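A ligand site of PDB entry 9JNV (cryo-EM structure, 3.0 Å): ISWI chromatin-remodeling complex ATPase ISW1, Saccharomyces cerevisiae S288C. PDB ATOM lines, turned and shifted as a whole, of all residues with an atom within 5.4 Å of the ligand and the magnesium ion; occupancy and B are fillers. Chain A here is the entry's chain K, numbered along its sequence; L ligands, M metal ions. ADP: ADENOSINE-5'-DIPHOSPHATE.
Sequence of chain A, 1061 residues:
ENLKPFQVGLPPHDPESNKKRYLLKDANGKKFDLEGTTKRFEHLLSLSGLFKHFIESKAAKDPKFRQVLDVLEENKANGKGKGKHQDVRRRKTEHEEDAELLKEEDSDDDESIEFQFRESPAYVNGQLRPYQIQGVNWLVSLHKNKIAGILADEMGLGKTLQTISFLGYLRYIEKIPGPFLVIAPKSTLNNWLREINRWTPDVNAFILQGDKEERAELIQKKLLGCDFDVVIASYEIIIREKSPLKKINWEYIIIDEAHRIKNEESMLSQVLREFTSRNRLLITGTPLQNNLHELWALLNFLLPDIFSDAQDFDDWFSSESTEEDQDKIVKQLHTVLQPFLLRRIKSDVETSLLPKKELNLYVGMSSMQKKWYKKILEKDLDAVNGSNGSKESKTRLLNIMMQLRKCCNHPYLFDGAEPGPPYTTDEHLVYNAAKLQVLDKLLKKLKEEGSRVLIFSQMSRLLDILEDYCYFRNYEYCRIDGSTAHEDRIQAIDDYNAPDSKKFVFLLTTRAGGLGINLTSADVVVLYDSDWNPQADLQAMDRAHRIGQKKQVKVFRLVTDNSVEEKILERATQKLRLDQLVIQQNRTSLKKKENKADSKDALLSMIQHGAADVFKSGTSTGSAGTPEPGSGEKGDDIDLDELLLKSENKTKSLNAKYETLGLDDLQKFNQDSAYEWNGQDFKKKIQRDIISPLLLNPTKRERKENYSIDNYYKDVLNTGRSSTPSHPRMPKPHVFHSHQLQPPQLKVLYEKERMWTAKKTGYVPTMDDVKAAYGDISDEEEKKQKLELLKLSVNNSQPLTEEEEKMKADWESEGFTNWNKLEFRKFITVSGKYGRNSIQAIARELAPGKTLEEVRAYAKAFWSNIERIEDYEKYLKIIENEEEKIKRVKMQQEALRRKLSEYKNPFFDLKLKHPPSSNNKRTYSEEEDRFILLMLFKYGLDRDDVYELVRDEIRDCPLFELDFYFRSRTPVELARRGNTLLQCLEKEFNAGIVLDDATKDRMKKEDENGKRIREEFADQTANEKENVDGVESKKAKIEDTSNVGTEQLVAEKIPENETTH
The side-chain amino group (NZ) of Lys 159 is in salt-bridge range of an oxygen (O3B) of the ligand (3.98 Å).
NH2 of Arg 129 sits close to N1 of the ligand (3.4 Å).
O2A of the ligand is in hydrogen-bond range of N of Gly 158, at 3.0 Å.
N6 of the ligand sits at hydrogen-bond distance from O of Gln 127 (3.3 Å).
O2A of the ligand is in hydrogen-bond range of N of Lys 159 (3.1 Å).
OG1 of Thr 160 sits close to O5' of the ligand, at 3.5 Å.
The indole nitrogen of Trp 199 is in hydrogen-bond range of the side-chain carboxylate of Glu 195 (2.8 Å).
The backbone carbonyl oxygen of Gly 158 sits close to the side-chain amide oxygen of Gln 132 (3.2 Å).
The side-chain carboxylate (OD2) of Asp 256 lies close to the indole nitrogen (NE1) of Trp 192, at 3.3 Å.
OG1 of Thr 160 is in hydrogen-bond range of OE1 of Glu 195 (2.9 Å).
OE2 of Glu 257 lies close to O2B of the ligand (3.3 Å).
Leu 161 touches the ligand (CD2 to C6, 3.5 Å).
Trp 199 touches the ligand.
Hydrophobic or aromatic side chains that line the ligand: Leu 161 and Trp 199.
Merely in contact with the magnesium ion: Glu 257 (3.3 Å).
Two residues have an atom within 4 Å of the magnesium ion: Asp 256 and Glu 257.
The nearest printed residue that does not touch the magnesium ion is Thr 160 (4.2 Å).
The magnesium ion is bound by O2B of the ligand (2.0 Å) and OD2 of Asp 256 (2.1 Å).
Slightly farther from the magnesium ion lies the side-chain carboxylate (OD1) of Asp 256 (2.8 Å).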
ATOM      1  N   GLN A 127       3.613  -9.714 -10.404  1.00  0.00           N
ATOM      2  CA  GLN A 127       2.539  -9.554 -11.371  1.00  0.00           C
ATOM      3  C   GLN A 127       1.680 -10.806 -11.369  1.00  0.00           C
ATOM      4  O   GLN A 127       2.162 -11.919 -11.142  1.00  0.00           O
ATOM      5  CB  GLN A 127       3.098  -9.295 -12.776  1.00  0.00           C
ATOM      6  CG  GLN A 127       2.043  -8.987 -13.803  1.00  0.00           C
ATOM      7  CD  GLN A 127       0.974  -8.058 -13.264  1.00  0.00           C
ATOM      8  OE1 GLN A 127      -0.175  -8.448 -13.105  1.00  0.00           O
ATOM      9  NE2 GLN A 127       1.357  -6.818 -12.970  1.00  0.00           N
ATOM     10  N   LEU A 128       0.394 -10.618 -11.619  1.00  0.00           N
ATOM     11  CA  LEU A 128      -0.576 -11.705 -11.651  1.00  0.00           C
ATOM     12  C   LEU A 128      -1.231 -11.783 -13.018  1.00  0.00           C
ATOM     13  O   LEU A 128      -1.672 -10.764 -13.561  1.00  0.00           O
ATOM     14  CB  LEU A 128      -1.629 -11.508 -10.571  1.00  0.00           C
ATOM     15  CG  LEU A 128      -1.185 -11.953  -9.187  1.00  0.00           C
ATOM     16  CD1 LEU A 128      -2.358 -12.007  -8.242  1.00  0.00           C
ATOM     17  CD2 LEU A 128      -0.540 -13.303  -9.325  1.00  0.00           C
ATOM     18  N   ARG A 129      -1.286 -12.979 -13.560  1.00  0.00           N
ATOM     19  CA  ARG A 129      -1.997 -13.243 -14.796  1.00  0.00           C
ATOM     20  C   ARG A 129      -3.497 -13.279 -14.527  1.00  0.00           C
ATOM     21  O   ARG A 129      -3.930 -13.665 -13.442  1.00  0.00           O
ATOM     22  CB  ARG A 129      -1.506 -14.552 -15.396  1.00  0.00           C
ATOM     23  CG  ARG A 129      -1.736 -15.728 -14.500  1.00  0.00           C
ATOM     24  CD  ARG A 129      -0.946 -16.926 -14.953  1.00  0.00           C
ATOM     25  NE  ARG A 129       0.477 -16.718 -14.735  1.00  0.00           N
ATOM     26  CZ  ARG A 129       1.425 -17.588 -15.091  1.00  0.00           C
ATOM     27  NH1 ARG A 129       1.090 -18.721 -15.676  1.00  0.00           N
ATOM     28  NH2 ARG A 129       2.696 -17.306 -14.852  1.00  0.00           N
ATOM     29  N   GLN A 132      -5.670 -15.472 -12.185  1.00  0.00           N
ATOM     30  CA  GLN A 132      -5.248 -15.378 -10.794  1.00  0.00           C
ATOM     31  C   GLN A 132      -6.019 -14.282 -10.071  1.00  0.00           C
ATOM     32  O   GLN A 132      -6.571 -14.496  -8.991  1.00  0.00           O
ATOM     33  CB  GLN A 132      -3.739 -15.103 -10.726  1.00  0.00           C
ATOM     34  CG  GLN A 132      -2.854 -16.210 -11.244  1.00  0.00           C
ATOM     35  CD  GLN A 132      -2.703 -17.344 -10.268  1.00  0.00           C
ATOM     36  OE1 GLN A 132      -2.010 -17.223  -9.264  1.00  0.00           O
ATOM     37  NE2 GLN A 132      -3.340 -18.472 -10.555  1.00  0.00           N
ATOM     38  N   GLU A 154      -6.825 -26.439 -11.945  1.00  0.00           N
ATOM     39  CA  GLU A 154      -5.947 -27.467 -12.488  1.00  0.00           C
ATOM     40  C   GLU A 154      -4.528 -27.270 -11.966  1.00  0.00           C
ATOM     41  O   GLU A 154      -4.109 -26.161 -11.631  1.00  0.00           O
ATOM     42  CB  GLU A 154      -5.968 -27.427 -14.017  1.00  0.00           C
ATOM     43  CG  GLU A 154      -5.168 -28.541 -14.685  1.00  0.00           C
ATOM     44  CD  GLU A 154      -5.336 -28.565 -16.192  1.00  0.00           C
ATOM     45  OE1 GLU A 154      -6.284 -27.941 -16.708  1.00  0.00           O
ATOM     46  OE2 GLU A 154      -4.504 -29.208 -16.859  1.00  0.00           O
ATOM     47  N   MET A 155      -3.785 -28.381 -11.872  1.00  0.00           N
ATOM     48  CA  MET A 155      -2.441 -28.331 -11.318  1.00  0.00           C
ATOM     49  C   MET A 155      -1.526 -27.484 -12.176  1.00  0.00           C
ATOM     50  O   MET A 155      -1.667 -27.415 -13.395  1.00  0.00           O
ATOM     51  CB  MET A 155      -1.871 -29.740 -11.189  1.00  0.00           C
ATOM     52  CG  MET A 155      -2.577 -30.599 -10.170  1.00  0.00           C
ATOM     53  SD  MET A 155      -1.888 -32.255 -10.148  1.00  0.00           S
ATOM     54  CE  MET A 155      -0.304 -31.913  -9.403  1.00  0.00           C
ATOM     55  N   GLY A 156      -0.572 -26.825 -11.519  1.00  0.00           N
ATOM     56  CA  GLY A 156       0.340 -25.939 -12.210  1.00  0.00           C
ATOM     57  C   GLY A 156      -0.198 -24.555 -12.459  1.00  0.00           C
ATOM     58  O   GLY A 156       0.522 -23.712 -12.997  1.00  0.00           O
ATOM     59  N   LEU A 157      -1.441 -24.295 -12.069  1.00  0.00           N
ATOM     60  CA  LEU A 157      -2.071 -23.003 -12.312  1.00  0.00           C
ATOM     61  C   LEU A 157      -1.695 -21.975 -11.257  1.00  0.00           C
ATOM     62  O   LEU A 157      -2.175 -20.833 -11.332  1.00  0.00           O
ATOM     63  CB  LEU A 157      -3.588 -23.165 -12.367  1.00  0.00           C
ATOM     64  CG  LEU A 157      -4.228 -23.573 -13.700  1.00  0.00           C
ATOM     65  CD1 LEU A 157      -4.161 -22.472 -14.716  1.00  0.00           C
ATOM     66  CD2 LEU A 157      -3.551 -24.805 -14.272  1.00  0.00           C
ATOM     67  N   GLY A 158      -0.885 -22.341 -10.275  1.00  0.00           N
ATOM     68  CA  GLY A 158      -0.404 -21.401  -9.294  1.00  0.00           C
ATOM     69  C   GLY A 158      -1.385 -21.125  -8.183  1.00  0.00           C
ATOM     70  O   GLY A 158      -1.584 -19.979  -7.776  1.00  0.00           O
ATOM     71  N   LYS A 159      -2.015 -22.184  -7.683  1.00  0.00           N
ATOM     72  CA  LYS A 159      -3.082 -22.000  -6.707  1.00  0.00           C
ATOM     73  C   LYS A 159      -2.562 -21.365  -5.424  1.00  0.00           C
ATOM     74  O   LYS A 159      -3.204 -20.465  -4.859  1.00  0.00           O
ATOM     75  CB  LYS A 159      -3.739 -23.344  -6.427  1.00  0.00           C
ATOM     76  CG  LYS A 159      -3.790 -24.225  -7.649  1.00  0.00           C
ATOM     77  CD  LYS A 159      -4.652 -25.436  -7.396  1.00  0.00           C
ATOM     78  CE  LYS A 159      -3.951 -26.450  -6.534  1.00  0.00           C
ATOM     79  NZ  LYS A 159      -4.687 -27.723  -6.486  1.00  0.00           N
ATOM     80  N   THR A 160      -1.405 -21.826  -4.949  1.00  0.00           N
ATOM     81  CA  THR A 160      -0.872 -21.284  -3.702  1.00  0.00           C
ATOM     82  C   THR A 160      -0.523 -19.815  -3.843  1.00  0.00           C
ATOM     83  O   THR A 160      -0.583 -19.070  -2.857  1.00  0.00           O
ATOM     84  CB  THR A 160       0.359 -22.073  -3.261  1.00  0.00           C
ATOM     85  OG1 THR A 160       1.384 -21.945  -4.244  1.00  0.00           O
ATOM     86  CG2 THR A 160       0.012 -23.535  -3.088  1.00  0.00           C
ATOM     87  N   LEU A 161      -0.141 -19.365  -5.028  1.00  0.00           N
ATOM     88  CA  LEU A 161       0.029 -17.936  -5.230  1.00  0.00           C
ATOM     89  C   LEU A 161      -1.278 -17.188  -5.031  1.00  0.00           C
ATOM     90  O   LEU A 161      -1.304 -16.116  -4.437  1.00  0.00           O
ATOM     91  CB  LEU A 161       0.603 -17.666  -6.613  1.00  0.00           C
ATOM     92  CG  LEU A 161       0.821 -16.182  -6.811  1.00  0.00           C
ATOM     93  CD1 LEU A 161       1.800 -15.679  -5.814  1.00  0.00           C
ATOM     94  CD2 LEU A 161       1.360 -15.986  -8.208  1.00  0.00           C
ATOM     95  N   THR A 188       5.669 -30.806   0.178  1.00  0.00           N
ATOM     96  CA  THR A 188       5.508 -29.409  -0.180  1.00  0.00           C
ATOM     97  C   THR A 188       5.583 -28.484   1.023  1.00  0.00           C
ATOM     98  O   THR A 188       5.356 -27.284   0.874  1.00  0.00           O
ATOM     99  CB  THR A 188       4.192 -29.182  -0.893  1.00  0.00           C
ATOM    100  OG1 THR A 188       3.119 -29.539  -0.014  1.00  0.00           O
ATOM    101  CG2 THR A 188       4.123 -30.055  -2.125  1.00  0.00           C
ATOM    102  N   ASN A 191       7.868 -25.779   0.082  1.00  0.00           N
ATOM    103  CA  ASN A 191       7.440 -24.876  -0.986  1.00  0.00           C
ATOM    104  C   ASN A 191       6.560 -23.759  -0.449  1.00  0.00           C
ATOM    105  O   ASN A 191       6.690 -22.597  -0.861  1.00  0.00           O
ATOM    106  CB  ASN A 191       6.688 -25.667  -2.059  1.00  0.00           C
ATOM    107  CG  ASN A 191       6.361 -24.836  -3.273  1.00  0.00           C
ATOM    108  OD1 ASN A 191       6.695 -23.663  -3.347  1.00  0.00           O
ATOM    109  ND2 ASN A 191       5.687 -25.442  -4.232  1.00  0.00           N
ATOM    110  N   TRP A 192       5.635 -24.084   0.452  1.00  0.00           N
ATOM    111  CA  TRP A 192       4.780 -23.062   1.029  1.00  0.00           C
ATOM    112  C   TRP A 192       5.621 -21.936   1.613  1.00  0.00           C
ATOM    113  O   TRP A 192       5.380 -20.760   1.319  1.00  0.00           O
ATOM    114  CB  TRP A 192       3.904 -23.683   2.109  1.00  0.00           C
ATOM    115  CG  TRP A 192       2.566 -24.109   1.627  1.00  0.00           C
ATOM    116  CD1 TRP A 192       2.085 -25.379   1.564  1.00  0.00           C
ATOM    117  CD2 TRP A 192       1.525 -23.270   1.124  1.00  0.00           C
ATOM    118  NE1 TRP A 192       0.809 -25.384   1.060  1.00  0.00           N
ATOM    119  CE2 TRP A 192       0.445 -24.093   0.783  1.00  0.00           C
ATOM    120  CE3 TRP A 192       1.405 -21.887   0.930  1.00  0.00           C
ATOM    121  CZ2 TRP A 192      -0.731 -23.591   0.254  1.00  0.00           C
ATOM    122  CZ3 TRP A 192       0.246 -21.401   0.416  1.00  0.00           C
ATOM    123  CH2 TRP A 192      -0.813 -22.246   0.082  1.00  0.00           C
ATOM    124  N   GLU A 195       7.627 -19.780  -0.884  1.00  0.00           N
ATOM    125  CA  GLU A 195       6.864 -18.790  -1.617  1.00  0.00           C
ATOM    126  C   GLU A 195       6.246 -17.736  -0.719  1.00  0.00           C
ATOM    127  O   GLU A 195       6.052 -16.587  -1.152  1.00  0.00           O
ATOM    128  CB  GLU A 195       5.806 -19.483  -2.474  1.00  0.00           C
ATOM    129  CG  GLU A 195       5.040 -18.540  -3.311  1.00  0.00           C
ATOM    130  CD  GLU A 195       4.031 -19.212  -4.203  1.00  0.00           C
ATOM    131  OE1 GLU A 195       3.919 -20.448  -4.138  1.00  0.00           O
ATOM    132  OE2 GLU A 195       3.374 -18.492  -4.984  1.00  0.00           O
ATOM    133  N   ARG A 198       8.573 -15.277  -0.589  1.00  0.00           N
ATOM    134  CA  ARG A 198       8.882 -14.831  -1.935  1.00  0.00           C
ATOM    135  C   ARG A 198       7.963 -13.704  -2.398  1.00  0.00           C
ATOM    136  O   ARG A 198       8.452 -12.688  -2.899  1.00  0.00           O
ATOM    137  CB  ARG A 198       8.790 -16.013  -2.904  1.00  0.00           C
ATOM    138  CG  ARG A 198       9.621 -15.840  -4.147  1.00  0.00           C
ATOM    139  CD  ARG A 198       8.835 -15.144  -5.236  1.00  0.00           C
ATOM    140  NE  ARG A 198       9.402 -15.412  -6.550  1.00  0.00           N
ATOM    141  CZ  ARG A 198       9.033 -14.775  -7.646  1.00  0.00           C
ATOM    142  NH1 ARG A 198       8.108 -13.821  -7.563  1.00  0.00           N
ATOM    143  NH2 ARG A 198       9.576 -15.065  -8.821  1.00  0.00           N
ATOM    144  N   TRP A 199       6.653 -13.852  -2.249  1.00  0.00           N
ATOM    145  CA  TRP A 199       5.755 -12.791  -2.702  1.00  0.00           C
ATOM    146  C   TRP A 199       5.512 -11.747  -1.610  1.00  0.00           C
ATOM    147  O   TRP A 199       5.773 -10.558  -1.810  1.00  0.00           O
ATOM    148  CB  TRP A 199       4.444 -13.383  -3.185  1.00  0.00           C
ATOM    149  CG  TRP A 199       4.643 -14.312  -4.286  1.00  0.00           C
ATOM    150  CD1 TRP A 199       4.675 -15.655  -4.200  1.00  0.00           C
ATOM    151  CD2 TRP A 199       4.842 -13.987  -5.662  1.00  0.00           C
ATOM    152  NE1 TRP A 199       4.894 -16.204  -5.441  1.00  0.00           N
ATOM    153  CE2 TRP A 199       5.000 -15.198  -6.352  1.00  0.00           C
ATOM    154  CE3 TRP A 199       4.901 -12.794  -6.375  1.00  0.00           C
ATOM    155  CZ2 TRP A 199       5.203 -15.254  -7.726  1.00  0.00           C
ATOM    156  CZ3 TRP A 199       5.108 -12.848  -7.725  1.00  0.00           C
ATOM    157  CH2 TRP A 199       5.250 -14.067  -8.391  1.00  0.00           C
ATOM    158  N   ASP A 256      -3.890 -27.472   1.651  1.00  0.00           N
ATOM    159  CA  ASP A 256      -3.411 -27.889   0.343  1.00  0.00           C
ATOM    160  C   ASP A 256      -3.827 -29.324   0.085  1.00  0.00           C
ATOM    161  O   ASP A 256      -3.996 -30.120   1.009  1.00  0.00           O
ATOM    162  CB  ASP A 256      -1.909 -27.759   0.257  1.00  0.00           C
ATOM    163  CG  ASP A 256      -1.397 -27.825  -1.157  1.00  0.00           C
ATOM    164  OD1 ASP A 256      -1.972 -28.593  -1.956  1.00  0.00           O
ATOM    165  OD2 ASP A 256      -0.425 -27.118  -1.484  1.00  0.00           O
ATOM    166  N   GLU A 257      -3.976 -29.673  -1.197  1.00  0.00           N
ATOM    167  CA  GLU A 257      -4.407 -31.003  -1.617  1.00  0.00           C
ATOM    168  C   GLU A 257      -5.631 -31.450  -0.821  1.00  0.00           C
ATOM    169  O   GLU A 257      -5.586 -32.388  -0.028  1.00  0.00           O
ATOM    170  CB  GLU A 257      -3.275 -32.019  -1.487  1.00  0.00           C
ATOM    171  CG  GLU A 257      -2.015 -31.638  -2.209  1.00  0.00           C
ATOM    172  CD  GLU A 257      -2.258 -31.256  -3.645  1.00  0.00           C
ATOM    173  OE1 GLU A 257      -3.088 -31.908  -4.308  1.00  0.00           O
ATOM    174  OE2 GLU A 257      -1.601 -30.297  -4.114  1.00  0.00           O
HETATM  175  PB  ADP L   1       0.081 -27.144  -6.748  1.00  0.00           P
HETATM  176  O1B ADP L   1       0.879 -28.171  -7.506  1.00  0.00           O
HETATM  177  O2B ADP L   1      -0.274 -27.556  -5.351  1.00  0.00           O
HETATM  178  O3B ADP L   1      -1.036 -26.529  -7.533  1.00  0.00           O
HETATM  179  PA  ADP L   1       1.489 -24.949  -7.730  1.00  0.00           P
HETATM  180  O1A ADP L   1       2.407 -25.651  -8.687  1.00  0.00           O
HETATM  181  O2A ADP L   1       0.224 -24.276  -8.219  1.00  0.00           O
HETATM  182  O3A ADP L   1       1.113 -25.945  -6.527  1.00  0.00           O
HETATM  183  O5' ADP L   1       2.357 -23.836  -6.963  1.00  0.00           O
HETATM  184  C5' ADP L   1       2.291 -22.497  -7.404  1.00  0.00           C
HETATM  185  C4' ADP L   1       3.023 -22.461  -8.723  1.00  0.00           C
HETATM  186  O4' ADP L   1       2.780 -21.230  -9.386  1.00  0.00           O
HETATM  187  C3' ADP L   1       4.515 -22.541  -8.529  1.00  0.00           C
HETATM  188  O3' ADP L   1       4.923 -23.891  -8.672  1.00  0.00           O
HETATM  189  C2' ADP L   1       5.088 -21.682  -9.632  1.00  0.00           C
HETATM  190  O2' ADP L   1       5.651 -22.524 -10.637  1.00  0.00           O
HETATM  191  C1' ADP L   1       3.898 -20.951 -10.230  1.00  0.00           C
HETATM  192  N9  ADP L   1       4.141 -19.496 -10.272  1.00  0.00           N
HETATM  193  C8  ADP L   1       5.243 -18.872  -9.830  1.00  0.00           C
HETATM  194  N7  ADP L   1       5.159 -17.533 -10.035  1.00  0.00           N
HETATM  195  C5  ADP L   1       3.978 -17.287 -10.627  1.00  0.00           C
HETATM  196  C6  ADP L   1       3.251 -16.095 -11.124  1.00  0.00           C
HETATM  197  N6  ADP L   1       3.774 -14.853 -11.021  1.00  0.00           N
HETATM  198  N1  ADP L   1       2.034 -16.295 -11.673  1.00  0.00           N
HETATM  199  C2  ADP L   1       1.501 -17.516 -11.781  1.00  0.00           C
HETATM  200  N3  ADP L   1       2.099 -18.643 -11.357  1.00  0.00           N
HETATM  201  C4  ADP L   1       3.326 -18.595 -10.786  1.00  0.00           C
HETATM  202 MG    MG M   1       0.234 -27.677  -3.449  1.00  0.00          MG
